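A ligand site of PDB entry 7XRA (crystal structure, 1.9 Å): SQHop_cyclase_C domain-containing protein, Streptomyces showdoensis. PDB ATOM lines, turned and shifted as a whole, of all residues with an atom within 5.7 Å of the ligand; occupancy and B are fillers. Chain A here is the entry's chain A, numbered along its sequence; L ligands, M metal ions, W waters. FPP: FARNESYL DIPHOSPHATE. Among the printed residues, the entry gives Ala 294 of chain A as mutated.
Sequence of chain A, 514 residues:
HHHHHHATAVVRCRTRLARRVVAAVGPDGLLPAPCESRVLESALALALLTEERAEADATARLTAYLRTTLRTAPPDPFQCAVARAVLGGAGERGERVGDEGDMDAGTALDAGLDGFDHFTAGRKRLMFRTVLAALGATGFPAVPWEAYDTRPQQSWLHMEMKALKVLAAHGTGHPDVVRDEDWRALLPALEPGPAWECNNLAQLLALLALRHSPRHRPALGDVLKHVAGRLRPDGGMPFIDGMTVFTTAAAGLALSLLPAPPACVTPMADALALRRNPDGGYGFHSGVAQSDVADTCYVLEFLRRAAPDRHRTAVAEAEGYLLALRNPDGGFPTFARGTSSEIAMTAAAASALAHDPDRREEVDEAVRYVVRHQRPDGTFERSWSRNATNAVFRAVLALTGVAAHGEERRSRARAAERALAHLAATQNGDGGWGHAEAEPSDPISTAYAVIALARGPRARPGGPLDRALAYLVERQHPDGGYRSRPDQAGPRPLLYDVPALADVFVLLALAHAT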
ATOM      1  N   THR A 120       3.167  12.721  15.809  1.00  0.00           N
ATOM      2  CA  THR A 120       4.419  12.104  16.255  1.00  0.00           C
ATOM      3  C   THR A 120       4.570  10.657  15.813  1.00  0.00           C
ATOM      4  O   THR A 120       5.566  10.026  16.165  1.00  0.00           O
ATOM      5  CB  THR A 120       4.525  12.147  17.782  1.00  0.00           C
ATOM      6  OG1 THR A 120       3.497  11.338  18.369  1.00  0.00           O
ATOM      7  CG2 THR A 120       4.413  13.584  18.299  1.00  0.00           C
ATOM      8  N   ARG A 123       8.104   9.639  14.481  1.00  0.00           N
ATOM      9  CA  ARG A 123       9.093   9.603  15.554  1.00  0.00           C
ATOM     10  C   ARG A 123       8.878   8.398  16.458  1.00  0.00           C
ATOM     11  O   ARG A 123       9.841   7.751  16.888  1.00  0.00           O
ATOM     12  CB  ARG A 123       9.050  10.915  16.355  1.00  0.00           C
ATOM     13  CG  ARG A 123       9.834  10.891  17.662  1.00  0.00           C
ATOM     14  CD  ARG A 123      10.045  12.302  18.227  1.00  0.00           C
ATOM     15  NE  ARG A 123       8.807  12.949  18.673  1.00  0.00           N
ATOM     16  CZ  ARG A 123       8.219  12.718  19.838  1.00  0.00           C
ATOM     17  NH1 ARG A 123       8.685  11.804  20.679  1.00  0.00           N
ATOM     18  NH2 ARG A 123       7.149  13.429  20.174  1.00  0.00           N
ATOM     19  N   LYS A 124       7.608   8.074  16.760  1.00  0.00           N
ATOM     20  CA  LYS A 124       7.328   6.988  17.689  1.00  0.00           C
ATOM     21  C   LYS A 124       7.733   5.632  17.112  1.00  0.00           C
ATOM     22  O   LYS A 124       8.242   4.771  17.826  1.00  0.00           O
ATOM     23  CB  LYS A 124       5.855   6.972  18.064  1.00  0.00           C
ATOM     24  CG  LYS A 124       5.434   8.144  18.920  1.00  0.00           C
ATOM     25  CD  LYS A 124       6.205   8.167  20.216  1.00  0.00           C
ATOM     26  CE  LYS A 124       5.990   9.490  20.923  1.00  0.00           C
ATOM     27  NZ  LYS A 124       4.565   9.910  20.803  1.00  0.00           N
ATOM     28  N   MET A 127      11.456   5.506  17.543  1.00  0.00           N
ATOM     29  CA  MET A 127      11.783   5.306  18.949  1.00  0.00           C
ATOM     30  C   MET A 127      11.530   3.868  19.386  1.00  0.00           C
ATOM     31  O   MET A 127      12.417   3.192  19.923  1.00  0.00           O
ATOM     32  CB  MET A 127      10.965   6.253  19.835  1.00  0.00           C
ATOM     33  CG  MET A 127      11.357   7.719  19.802  1.00  0.00           C
ATOM     34  SD  MET A 127      10.294   8.699  20.898  1.00  0.00           S
ATOM     35  CE  MET A 127       9.985   7.496  22.210  1.00  0.00           C
ATOM     36  N   GLN A 154       9.977  19.315  24.545  1.00  0.00           N
ATOM     37  CA  GLN A 154      10.126  19.006  25.963  1.00  0.00           C
ATOM     38  C   GLN A 154      11.571  18.584  26.232  1.00  0.00           C
ATOM     39  O   GLN A 154      12.185  17.873  25.434  1.00  0.00           O
ATOM     40  CB  GLN A 154       9.156  17.914  26.411  1.00  0.00           C
ATOM     41  CG  GLN A 154       9.368  16.560  25.758  1.00  0.00           C
ATOM     42  CD  GLN A 154       8.465  16.341  24.560  1.00  0.00           C
ATOM     43  OE1 GLN A 154       8.442  17.160  23.639  1.00  0.00           O
ATOM     44  NE2 GLN A 154       7.719  15.247  24.566  1.00  0.00           N
ATOM     45  N   TRP A 156      13.276  16.539  28.203  1.00  0.00           N
ATOM     46  CA  TRP A 156      13.704  15.145  28.250  1.00  0.00           C
ATOM     47  C   TRP A 156      13.597  14.436  26.908  1.00  0.00           C
ATOM     48  O   TRP A 156      14.279  13.429  26.700  1.00  0.00           O
ATOM     49  CB  TRP A 156      12.891  14.380  29.301  1.00  0.00           C
ATOM     50  CG  TRP A 156      11.414  14.423  28.990  1.00  0.00           C
ATOM     51  CD1 TRP A 156      10.743  13.607  28.123  1.00  0.00           C
ATOM     52  CD2 TRP A 156      10.452  15.328  29.528  1.00  0.00           C
ATOM     53  NE1 TRP A 156       9.418  13.950  28.101  1.00  0.00           N
ATOM     54  CE2 TRP A 156       9.211  15.009  28.945  1.00  0.00           C
ATOM     55  CE3 TRP A 156      10.510  16.392  30.445  1.00  0.00           C
ATOM     56  CZ2 TRP A 156       8.037  15.694  29.251  1.00  0.00           C
ATOM     57  CZ3 TRP A 156       9.336  17.077  30.751  1.00  0.00           C
ATOM     58  CH2 TRP A 156       8.124  16.730  30.158  1.00  0.00           C
ATOM     59  N   LEU A 157      12.761  14.924  25.992  1.00  0.00           N
ATOM     60  CA  LEU A 157      12.624  14.256  24.688  1.00  0.00           C
ATOM     61  C   LEU A 157      13.928  14.316  23.893  1.00  0.00           C
ATOM     62  O   LEU A 157      14.289  13.353  23.215  1.00  0.00           O
ATOM     63  CB  LEU A 157      11.498  14.878  23.882  1.00  0.00           C
ATOM     64  CG  LEU A 157      11.545  14.383  22.434  1.00  0.00           C
ATOM     65  CD1 LEU A 157      11.270  12.894  22.395  1.00  0.00           C
ATOM     66  CD2 LEU A 157      10.608  15.156  21.519  1.00  0.00           C
ATOM     67  N   GLU A 160      16.016  11.442  25.272  1.00  0.00           N
ATOM     68  CA  GLU A 160      15.608  10.118  24.820  1.00  0.00           C
ATOM     69  C   GLU A 160      16.064   9.841  23.391  1.00  0.00           C
ATOM     70  O   GLU A 160      16.566   8.751  23.095  1.00  0.00           O
ATOM     71  CB  GLU A 160      14.080   9.970  24.917  1.00  0.00           C
ATOM     72  CG  GLU A 160      13.521  10.152  26.307  1.00  0.00           C
ATOM     73  CD  GLU A 160      12.020  10.366  26.278  1.00  0.00           C
ATOM     74  OE1 GLU A 160      11.504  10.780  25.213  1.00  0.00           O
ATOM     75  OE2 GLU A 160      11.369  10.124  27.307  1.00  0.00           O
ATOM     76  N   ASN A 199      11.373  11.952  35.243  1.00  0.00           N
ATOM     77  CA  ASN A 199      11.070  11.058  34.129  1.00  0.00           C
ATOM     78  C   ASN A 199      12.035   9.878  34.185  1.00  0.00           C
ATOM     79  O   ASN A 199      13.197   9.992  33.790  1.00  0.00           O
ATOM     80  CB  ASN A 199      11.162  11.805  32.805  1.00  0.00           C
ATOM     81  CG  ASN A 199      10.593  11.002  31.640  1.00  0.00           C
ATOM     82  OD1 ASN A 199      10.787   9.782  31.549  1.00  0.00           O
ATOM     83  ND2 ASN A 199       9.889  11.675  30.753  1.00  0.00           N
ATOM     84  N   LEU A 201      11.774   7.044  32.477  1.00  0.00           N
ATOM     85  CA  LEU A 201      12.012   6.482  31.154  1.00  0.00           C
ATOM     86  C   LEU A 201      13.207   7.156  30.504  1.00  0.00           C
ATOM     87  O   LEU A 201      14.110   6.486  29.978  1.00  0.00           O
ATOM     88  CB  LEU A 201      10.764   6.633  30.285  1.00  0.00           C
ATOM     89  CG  LEU A 201      10.933   6.291  28.794  1.00  0.00           C
ATOM     90  CD1 LEU A 201      11.395   4.846  28.617  1.00  0.00           C
ATOM     91  CD2 LEU A 201       9.629   6.526  28.028  1.00  0.00           C
ATOM     92  N   PHE A 239       6.720   5.163  35.485  1.00  0.00           N
ATOM     93  CA  PHE A 239       7.123   6.067  34.406  1.00  0.00           C
ATOM     94  C   PHE A 239       7.675   7.383  34.968  1.00  0.00           C
ATOM     95  O   PHE A 239       8.769   7.811  34.617  1.00  0.00           O
ATOM     96  CB  PHE A 239       5.928   6.291  33.471  1.00  0.00           C
ATOM     97  CG  PHE A 239       6.115   7.394  32.457  1.00  0.00           C
ATOM     98  CD1 PHE A 239       7.319   7.569  31.792  1.00  0.00           C
ATOM     99  CD2 PHE A 239       5.060   8.231  32.130  1.00  0.00           C
ATOM    100  CE1 PHE A 239       7.474   8.579  30.854  1.00  0.00           C
ATOM    101  CE2 PHE A 239       5.200   9.234  31.199  1.00  0.00           C
ATOM    102  CZ  PHE A 239       6.417   9.406  30.559  1.00  0.00           C
ATOM    103  N   ILE A 240       6.914   8.022  35.856  1.00  0.00           N
ATOM    104  CA  ILE A 240       7.302   9.312  36.426  1.00  0.00           C
ATOM    105  C   ILE A 240       7.219   9.215  37.935  1.00  0.00           C
ATOM    106  O   ILE A 240       6.561   8.332  38.500  1.00  0.00           O
ATOM    107  CB  ILE A 240       6.420  10.463  35.908  1.00  0.00           C
ATOM    108  CG1 ILE A 240       4.933  10.099  36.053  1.00  0.00           C
ATOM    109  CG2 ILE A 240       6.781  10.808  34.482  1.00  0.00           C
ATOM    110  CD1 ILE A 240       3.972  11.175  35.558  1.00  0.00           C
ATOM    111  N   MET A 243       2.572  13.085  39.714  1.00  0.00           N
ATOM    112  CA  MET A 243       1.883  14.078  38.909  1.00  0.00           C
ATOM    113  C   MET A 243       1.122  15.057  39.785  1.00  0.00           C
ATOM    114  O   MET A 243      -0.033  15.406  39.518  1.00  0.00           O
ATOM    115  CB  MET A 243       0.942  13.369  37.921  1.00  0.00           C
ATOM    116  CG  MET A 243       0.850  14.044  36.602  1.00  0.00           C
ATOM    117  SD  MET A 243      -0.246  13.140  35.493  1.00  0.00           S
ATOM    118  CE  MET A 243      -0.302  14.293  34.129  1.00  0.00           C
ATOM    119  N   PHE A 246      -0.407  18.701  38.238  1.00  0.00           N
ATOM    120  CA  PHE A 246      -1.586  18.485  37.413  1.00  0.00           C
ATOM    121  C   PHE A 246      -2.771  18.023  38.262  1.00  0.00           C
ATOM    122  O   PHE A 246      -3.884  18.526  38.113  1.00  0.00           O
ATOM    123  CB  PHE A 246      -1.252  17.449  36.323  1.00  0.00           C
ATOM    124  CG  PHE A 246      -2.373  17.184  35.358  1.00  0.00           C
ATOM    125  CD1 PHE A 246      -2.668  18.093  34.357  1.00  0.00           C
ATOM    126  CD2 PHE A 246      -3.122  16.012  35.428  1.00  0.00           C
ATOM    127  CE1 PHE A 246      -3.699  17.850  33.445  1.00  0.00           C
ATOM    128  CE2 PHE A 246      -4.140  15.762  34.524  1.00  0.00           C
ATOM    129  CZ  PHE A 246      -4.422  16.674  33.541  1.00  0.00           C
ATOM    130  N   PHE A 284       4.284  19.175  35.470  1.00  0.00           N
ATOM    131  CA  PHE A 284       3.285  18.220  35.936  1.00  0.00           C
ATOM    132  C   PHE A 284       3.520  17.743  37.352  1.00  0.00           C
ATOM    133  O   PHE A 284       2.588  17.216  37.976  1.00  0.00           O
ATOM    134  CB  PHE A 284       3.222  17.013  34.995  1.00  0.00           C
ATOM    135  CG  PHE A 284       4.520  16.232  34.893  1.00  0.00           C
ATOM    136  CD1 PHE A 284       4.787  15.184  35.762  1.00  0.00           C
ATOM    137  CD2 PHE A 284       5.439  16.509  33.884  1.00  0.00           C
ATOM    138  CE1 PHE A 284       5.943  14.454  35.659  1.00  0.00           C
ATOM    139  CE2 PHE A 284       6.609  15.786  33.774  1.00  0.00           C
ATOM    140  CZ  PHE A 284       6.861  14.752  34.670  1.00  0.00           C
ATOM    141  N   ASP A 292       4.230  23.211  30.678  1.00  0.00           N
ATOM    142  CA  ASP A 292       3.373  22.757  29.578  1.00  0.00           C
ATOM    143  C   ASP A 292       1.998  23.416  29.671  1.00  0.00           C
ATOM    144  O   ASP A 292       1.555  23.830  30.735  1.00  0.00           O
ATOM    145  CB  ASP A 292       3.245  21.225  29.562  1.00  0.00           C
ATOM    146  CG  ASP A 292       2.358  20.703  30.659  1.00  0.00           C
ATOM    147  OD1 ASP A 292       1.115  20.675  30.459  1.00  0.00           O
ATOM    148  OD2 ASP A 292       2.888  20.320  31.713  1.00  0.00           O
ATOM    149  N   ALA A 294      -1.035  22.150  29.289  1.00  0.00           N
ATOM    150  CA  ALA A 294      -2.085  21.427  30.010  1.00  0.00           C
ATOM    151  C   ALA A 294      -2.063  21.772  31.499  1.00  0.00           C
ATOM    152  O   ALA A 294      -3.074  22.189  32.070  1.00  0.00           O
ATOM    153  CB  ALA A 294      -1.933  19.920  29.799  1.00  0.00           C
ATOM    154  N   ASP A 295      -0.916  21.551  32.147  1.00  0.00           N
ATOM    155  CA  ASP A 295      -0.769  21.931  33.553  1.00  0.00           C
ATOM    156  C   ASP A 295      -1.083  23.409  33.755  1.00  0.00           C
ATOM    157  O   ASP A 295      -1.830  23.777  34.664  1.00  0.00           O
ATOM    158  CB  ASP A 295       0.651  21.626  34.027  1.00  0.00           C
ATOM    159  CG  ASP A 295       0.836  20.178  34.366  1.00  0.00           C
ATOM    160  OD1 ASP A 295       0.278  19.746  35.386  1.00  0.00           O
ATOM    161  OD2 ASP A 295       1.547  19.474  33.607  1.00  0.00           O
ATOM    162  N   THR A 334       1.890  21.817  22.945  1.00  0.00           N
ATOM    163  CA  THR A 334       1.949  21.383  24.337  1.00  0.00           C
ATOM    164  C   THR A 334       3.095  22.052  25.078  1.00  0.00           C
ATOM    165  O   THR A 334       2.924  22.538  26.196  1.00  0.00           O
ATOM    166  CB  THR A 334       2.091  19.868  24.434  1.00  0.00           C
ATOM    167  OG1 THR A 334       0.959  19.231  23.834  1.00  0.00           O
ATOM    168  CG2 THR A 334       2.181  19.435  25.898  1.00  0.00           C
ATOM    169  N   PHE A 335       4.276  22.075  24.461  1.00  0.00           N
ATOM    170  CA  PHE A 335       5.505  22.475  25.133  1.00  0.00           C
ATOM    171  C   PHE A 335       6.214  23.669  24.519  1.00  0.00           C
ATOM    172  O   PHE A 335       6.843  24.427  25.248  1.00  0.00           O
ATOM    173  CB  PHE A 335       6.521  21.325  25.151  1.00  0.00           C
ATOM    174  CG  PHE A 335       6.067  20.110  25.895  1.00  0.00           C
ATOM    175  CD1 PHE A 335       6.068  20.067  27.280  1.00  0.00           C
ATOM    176  CD2 PHE A 335       5.685  18.964  25.213  1.00  0.00           C
ATOM    177  CE1 PHE A 335       5.673  18.941  27.974  1.00  0.00           C
ATOM    178  CE2 PHE A 335       5.298  17.830  25.886  1.00  0.00           C
ATOM    179  CZ  PHE A 335       5.285  17.810  27.265  1.00  0.00           C
ATOM    180  N   MET A 345      -5.036  21.171  23.626  1.00  0.00           N
ATOM    181  CA  MET A 345      -4.280  22.278  24.208  1.00  0.00           C
ATOM    182  C   MET A 345      -4.827  23.622  23.752  1.00  0.00           C
ATOM    183  O   MET A 345      -4.838  24.601  24.517  1.00  0.00           O
ATOM    184  CB  MET A 345      -2.799  22.172  23.829  1.00  0.00           C
ATOM    185  CG  MET A 345      -2.124  20.880  24.258  1.00  0.00           C
ATOM    186  SD  MET A 345      -2.003  20.653  26.054  1.00  0.00           S
ATOM    187  CE  MET A 345      -2.670  22.156  26.727  1.00  0.00           C
ATOM    188  N   TRP A 384      -2.743  13.343  24.475  1.00  0.00           N
ATOM    189  CA  TRP A 384      -2.291  12.928  25.797  1.00  0.00           C
ATOM    190  C   TRP A 384      -3.304  12.039  26.502  1.00  0.00           C
ATOM    191  O   TRP A 384      -2.931  11.236  27.374  1.00  0.00           O
ATOM    192  CB  TRP A 384      -1.967  14.169  26.633  1.00  0.00           C
ATOM    193  CG  TRP A 384      -0.887  15.008  26.007  1.00  0.00           C
ATOM    194  CD1 TRP A 384      -1.036  16.224  25.411  1.00  0.00           C
ATOM    195  CD2 TRP A 384       0.508  14.666  25.897  1.00  0.00           C
ATOM    196  NE1 TRP A 384       0.184  16.685  24.960  1.00  0.00           N
ATOM    197  CE2 TRP A 384       1.143  15.738  25.233  1.00  0.00           C
ATOM    198  CE3 TRP A 384       1.270  13.566  26.291  1.00  0.00           C
ATOM    199  CZ2 TRP A 384       2.518  15.738  24.962  1.00  0.00           C
ATOM    200  CZ3 TRP A 384       2.631  13.567  26.019  1.00  0.00           C
ATOM    201  CH2 TRP A 384       3.236  14.649  25.364  1.00  0.00           C
ATOM    202  N   GLN A 488      -4.251   8.519  30.547  1.00  0.00           N
ATOM    203  CA  GLN A 488      -3.089   9.335  30.219  1.00  0.00           C
ATOM    204  C   GLN A 488      -2.040   8.496  29.501  1.00  0.00           C
ATOM    205  O   GLN A 488      -1.780   7.351  29.882  1.00  0.00           O
ATOM    206  CB  GLN A 488      -2.496   9.950  31.484  1.00  0.00           C
ATOM    207  CG  GLN A 488      -3.441  10.891  32.234  1.00  0.00           C
ATOM    208  CD  GLN A 488      -3.749  12.137  31.451  1.00  0.00           C
ATOM    209  OE1 GLN A 488      -2.992  12.520  30.547  1.00  0.00           O
ATOM    210  NE2 GLN A 488      -4.868  12.791  31.773  1.00  0.00           N
ATOM    211  N   ALA A 489      -1.433   9.081  28.476  1.00  0.00           N
ATOM    212  CA  ALA A 489      -0.401   8.438  27.681  1.00  0.00           C
ATOM    213  C   ALA A 489       0.884   9.256  27.691  1.00  0.00           C
ATOM    214  O   ALA A 489       0.860  10.481  27.767  1.00  0.00           O
ATOM    215  CB  ALA A 489      -0.865   8.223  26.235  1.00  0.00           C
ATOM    216  N   GLY A 490       2.005   8.562  27.579  1.00  0.00           N
ATOM    217  CA  GLY A 490       3.293   9.211  27.541  1.00  0.00           C
ATOM    218  C   GLY A 490       4.402   8.192  27.672  1.00  0.00           C
ATOM    219  O   GLY A 490       4.430   7.399  28.617  1.00  0.00           O
ATOM    220  N   PRO A 491       5.299   8.138  26.695  1.00  0.00           N
ATOM    221  CA  PRO A 491       5.135   8.810  25.396  1.00  0.00           C
ATOM    222  C   PRO A 491       3.902   8.281  24.686  1.00  0.00           C
ATOM    223  O   PRO A 491       3.550   7.105  24.855  1.00  0.00           O
ATOM    224  CB  PRO A 491       6.404   8.422  24.632  1.00  0.00           C
ATOM    225  CG  PRO A 491       6.909   7.202  25.326  1.00  0.00           C
ATOM    226  CD  PRO A 491       6.538   7.346  26.758  1.00  0.00           C
ATOM    227  N   ARG A 492       3.248   9.125  23.907  1.00  0.00           N
ATOM    228  CA  ARG A 492       2.009   8.706  23.286  1.00  0.00           C
ATOM    229  C   ARG A 492       2.282   7.595  22.274  1.00  0.00           C
ATOM    230  O   ARG A 492       3.259   7.675  21.521  1.00  0.00           O
ATOM    231  CB  ARG A 492       1.341   9.900  22.601  1.00  0.00           C
ATOM    232  CG  ARG A 492       0.843  10.972  23.579  1.00  0.00           C
ATOM    233  CD  ARG A 492       0.677  12.344  22.908  1.00  0.00           C
ATOM    234  NE  ARG A 492       1.961  12.943  22.562  1.00  0.00           N
ATOM    235  CZ  ARG A 492       2.122  14.187  22.131  1.00  0.00           C
ATOM    236  NH1 ARG A 492       1.080  14.991  21.953  1.00  0.00           N
ATOM    237  NH2 ARG A 492       3.339  14.639  21.864  1.00  0.00           N
ATOM    238  N   TYR A 496      -0.082   5.308  31.073  1.00  0.00           N
ATOM    239  CA  TYR A 496       0.481   5.206  32.419  1.00  0.00           C
ATOM    240  C   TYR A 496      -0.624   5.553  33.413  1.00  0.00           C
ATOM    241  O   TYR A 496      -1.613   6.189  33.066  1.00  0.00           O
ATOM    242  CB  TYR A 496       1.706   6.116  32.608  1.00  0.00           C
ATOM    243  CG  TYR A 496       1.425   7.599  32.474  1.00  0.00           C
ATOM    244  CD1 TYR A 496       1.041   8.352  33.584  1.00  0.00           C
ATOM    245  CD2 TYR A 496       1.568   8.251  31.255  1.00  0.00           C
ATOM    246  CE1 TYR A 496       0.780   9.693  33.470  1.00  0.00           C
ATOM    247  CE2 TYR A 496       1.321   9.600  31.134  1.00  0.00           C
ATOM    248  CZ  TYR A 496       0.923  10.321  32.256  1.00  0.00           C
ATOM    249  OH  TYR A 496       0.653  11.671  32.162  1.00  0.00           O
HETATM  250  C1  FPP L   1       5.887  12.903  28.761  1.00  0.00           C
HETATM  251  O1  FPP L   1       5.394  12.567  27.474  1.00  0.00           O
HETATM  252  C2  FPP L   1       4.977  12.278  29.760  1.00  0.00           C
HETATM  253  C3  FPP L   1       4.752  12.780  30.972  1.00  0.00           C
HETATM  254  C4  FPP L   1       5.816  13.420  31.792  1.00  0.00           C
HETATM  255  C5  FPP L   1       3.393  12.707  31.601  1.00  0.00           C
HETATM  256  C6  FPP L   1       2.752  14.057  31.818  1.00  0.00           C
HETATM  257  C7  FPP L   1       2.375  14.714  30.521  1.00  0.00           C
HETATM  258  C8  FPP L   1       2.677  15.934  30.103  1.00  0.00           C
HETATM  259  C10 FPP L   1       3.581  16.874  30.852  1.00  0.00           C
HETATM  260  C9  FPP L   1       2.130  16.477  28.815  1.00  0.00           C
HETATM  261  C11 FPP L   1       0.647  16.270  28.626  1.00  0.00           C
HETATM  262  C12 FPP L   1      -0.175  16.812  29.749  1.00  0.00           C
HETATM  263  C13 FPP L   1      -0.340  16.312  30.959  1.00  0.00           C
HETATM  264  C14 FPP L   1      -1.163  15.091  31.212  1.00  0.00           C
HETATM  265  C15 FPP L   1       0.306  16.894  32.168  1.00  0.00           C
HETATM  266  PA  FPP L   1       6.423  12.267  26.301  1.00  0.00           P
HETATM  267  O1A FPP L   1       6.885  10.870  26.498  1.00  0.00           O
HETATM  268  O2A FPP L   1       7.413  13.365  26.243  1.00  0.00           O
HETATM  269  O3A FPP L   1       5.453  12.308  25.028  1.00  0.00           O
HETATM  270  PB  FPP L   1       5.592  12.125  23.438  1.00  0.00           P
HETATM  271  O1B FPP L   1       5.785  13.516  22.914  1.00  0.00           O
HETATM  272  O2B FPP L   1       4.323  11.513  22.991  1.00  0.00           O
HETATM  273  O3B FPP L   1       6.784  11.257  23.194  1.00  0.00           O
HETATM  274 MG    MG M   1       9.130  10.461  28.191  1.00  0.00          MG
HETATM  275 MG    MG M   2       9.249  10.894  24.613  1.00  0.00          MG
HETATM  276  O   HOH W   1      -0.391  12.344  29.626  1.00  0.00           O
HETATM  277  O   HOH W   2       5.548  19.350  32.217  1.00  0.00           O
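The side-chain sulfur (SD) of Met 243 sits close to the side-chain hydroxyl (OH) of Tyr 496, 3.7 Å away.
SD of Met 345 lies close to N of Ala 294, 3.7 Å away.
The guanidinium group (NH1) of Arg 123 lies within hydrogen-bond range of the side-chain sulfur (SD) of Met 127 (3.5 Å).
The backbone NH of Ala 489 lies within hydrogen-bond range of the backbone carbonyl oxygen of Trp 384 (2.8 Å).
The backbone NH (N) of Tyr 496 lies within hydrogen-bond range of the backbone carbonyl oxygen (O) of Gln 488, 2.9 Å away.
OD1 of Asp 292 sits at hydrogen-bond distance from N of Asp 295 (2.8 Å).
The side-chain carboxylate (OD2) of Asp 295 sits close to the backbone NH (N) of Phe 284 (3.3 Å).
O of Trp 384 lies close to OE1 of Gln 488 (3.4 Å).
The backbone nitrogen (N) of Pro 491 lies close to an oxygen (O1A) of the ligand (3.2 Å).
Phe 239 touches the ligand.
Ile 240 touches the ligand (CG2 to C4, 3.9 Å).
CE of Met 243 touches C14 of the ligand, 3.1 Å away.
CD1 of Phe 246 touches C15 of the ligand, 3.9 Å away.
Phe 284 touches the ligand (CE2 to C4, 3.2 Å).
Asp 292 touches the ligand.
Ala 294 touches the ligand.
Asp 295 touches the ligand (OD2 to C15, 3.2 Å).
CZ of Phe 335 touches C9 of the ligand, at 3.8 Å.
Trp 384 touches the ligand.
OE1 of Gln 488 touches C14 of the ligand, 3.2 Å away.
C of Gly 490 touches O1A of the ligand, at 3.8 Å.
Tyr 496 touches the ligand (OH to C5, 3.0 Å).
Hydrophobic or aromatic side chains that line the ligand: Trp 156, Phe 239, Ile 240, Met 243, Phe 246, Phe 284, Ala 294, Phe 335, Trp 384, Pro 491 and Tyr 496.
Within 4 Å of the ligand: Arg 123, Lys 124, Gln 154, Trp 156, Phe 239, Ile 240, Met 243, Phe 246, Phe 284, Asp 292, Ala 294, Asp 295, Phe 335, Trp 384, Gln 488, Gly 490, Pro 491, Arg 492 and Tyr 496.
The nearest printed residue that does not touch the ligand is Thr 334 (4.2 Å).
The side-chain amino group (NZ) of Lys 124 is in salt-bridge range of an oxygen (O2B) of the ligand (2.7 Å).
An oxygen (O2B) of the ligand is in salt-bridge range of the guanidinium group of Arg 492.
NE2 of Gln 154 is in hydrogen-bond range of O2A of the ligand (2.5 Å).
NH2 of Arg 123 lies within salt-bridge range of O1B of the ligand.
The indole nitrogen (NE1) of Trp 156 is in hydrogen-bond range of an oxygen (O2A) of the ligand (2.8 Å).
N of Arg 492 sits at hydrogen-bond distance from O2B of the ligand (2.8 Å).
Water W1 lies within hydrogen-bond range of the side-chain amide oxygen (OE1) of Gln 488, the side-chain hydroxyl (OH) of Tyr 496 and the backbone carbonyl oxygen (O) of Ala 489.
Water W2 lies within hydrogen-bond range of OD2 of Asp 292 and N of Phe 284.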
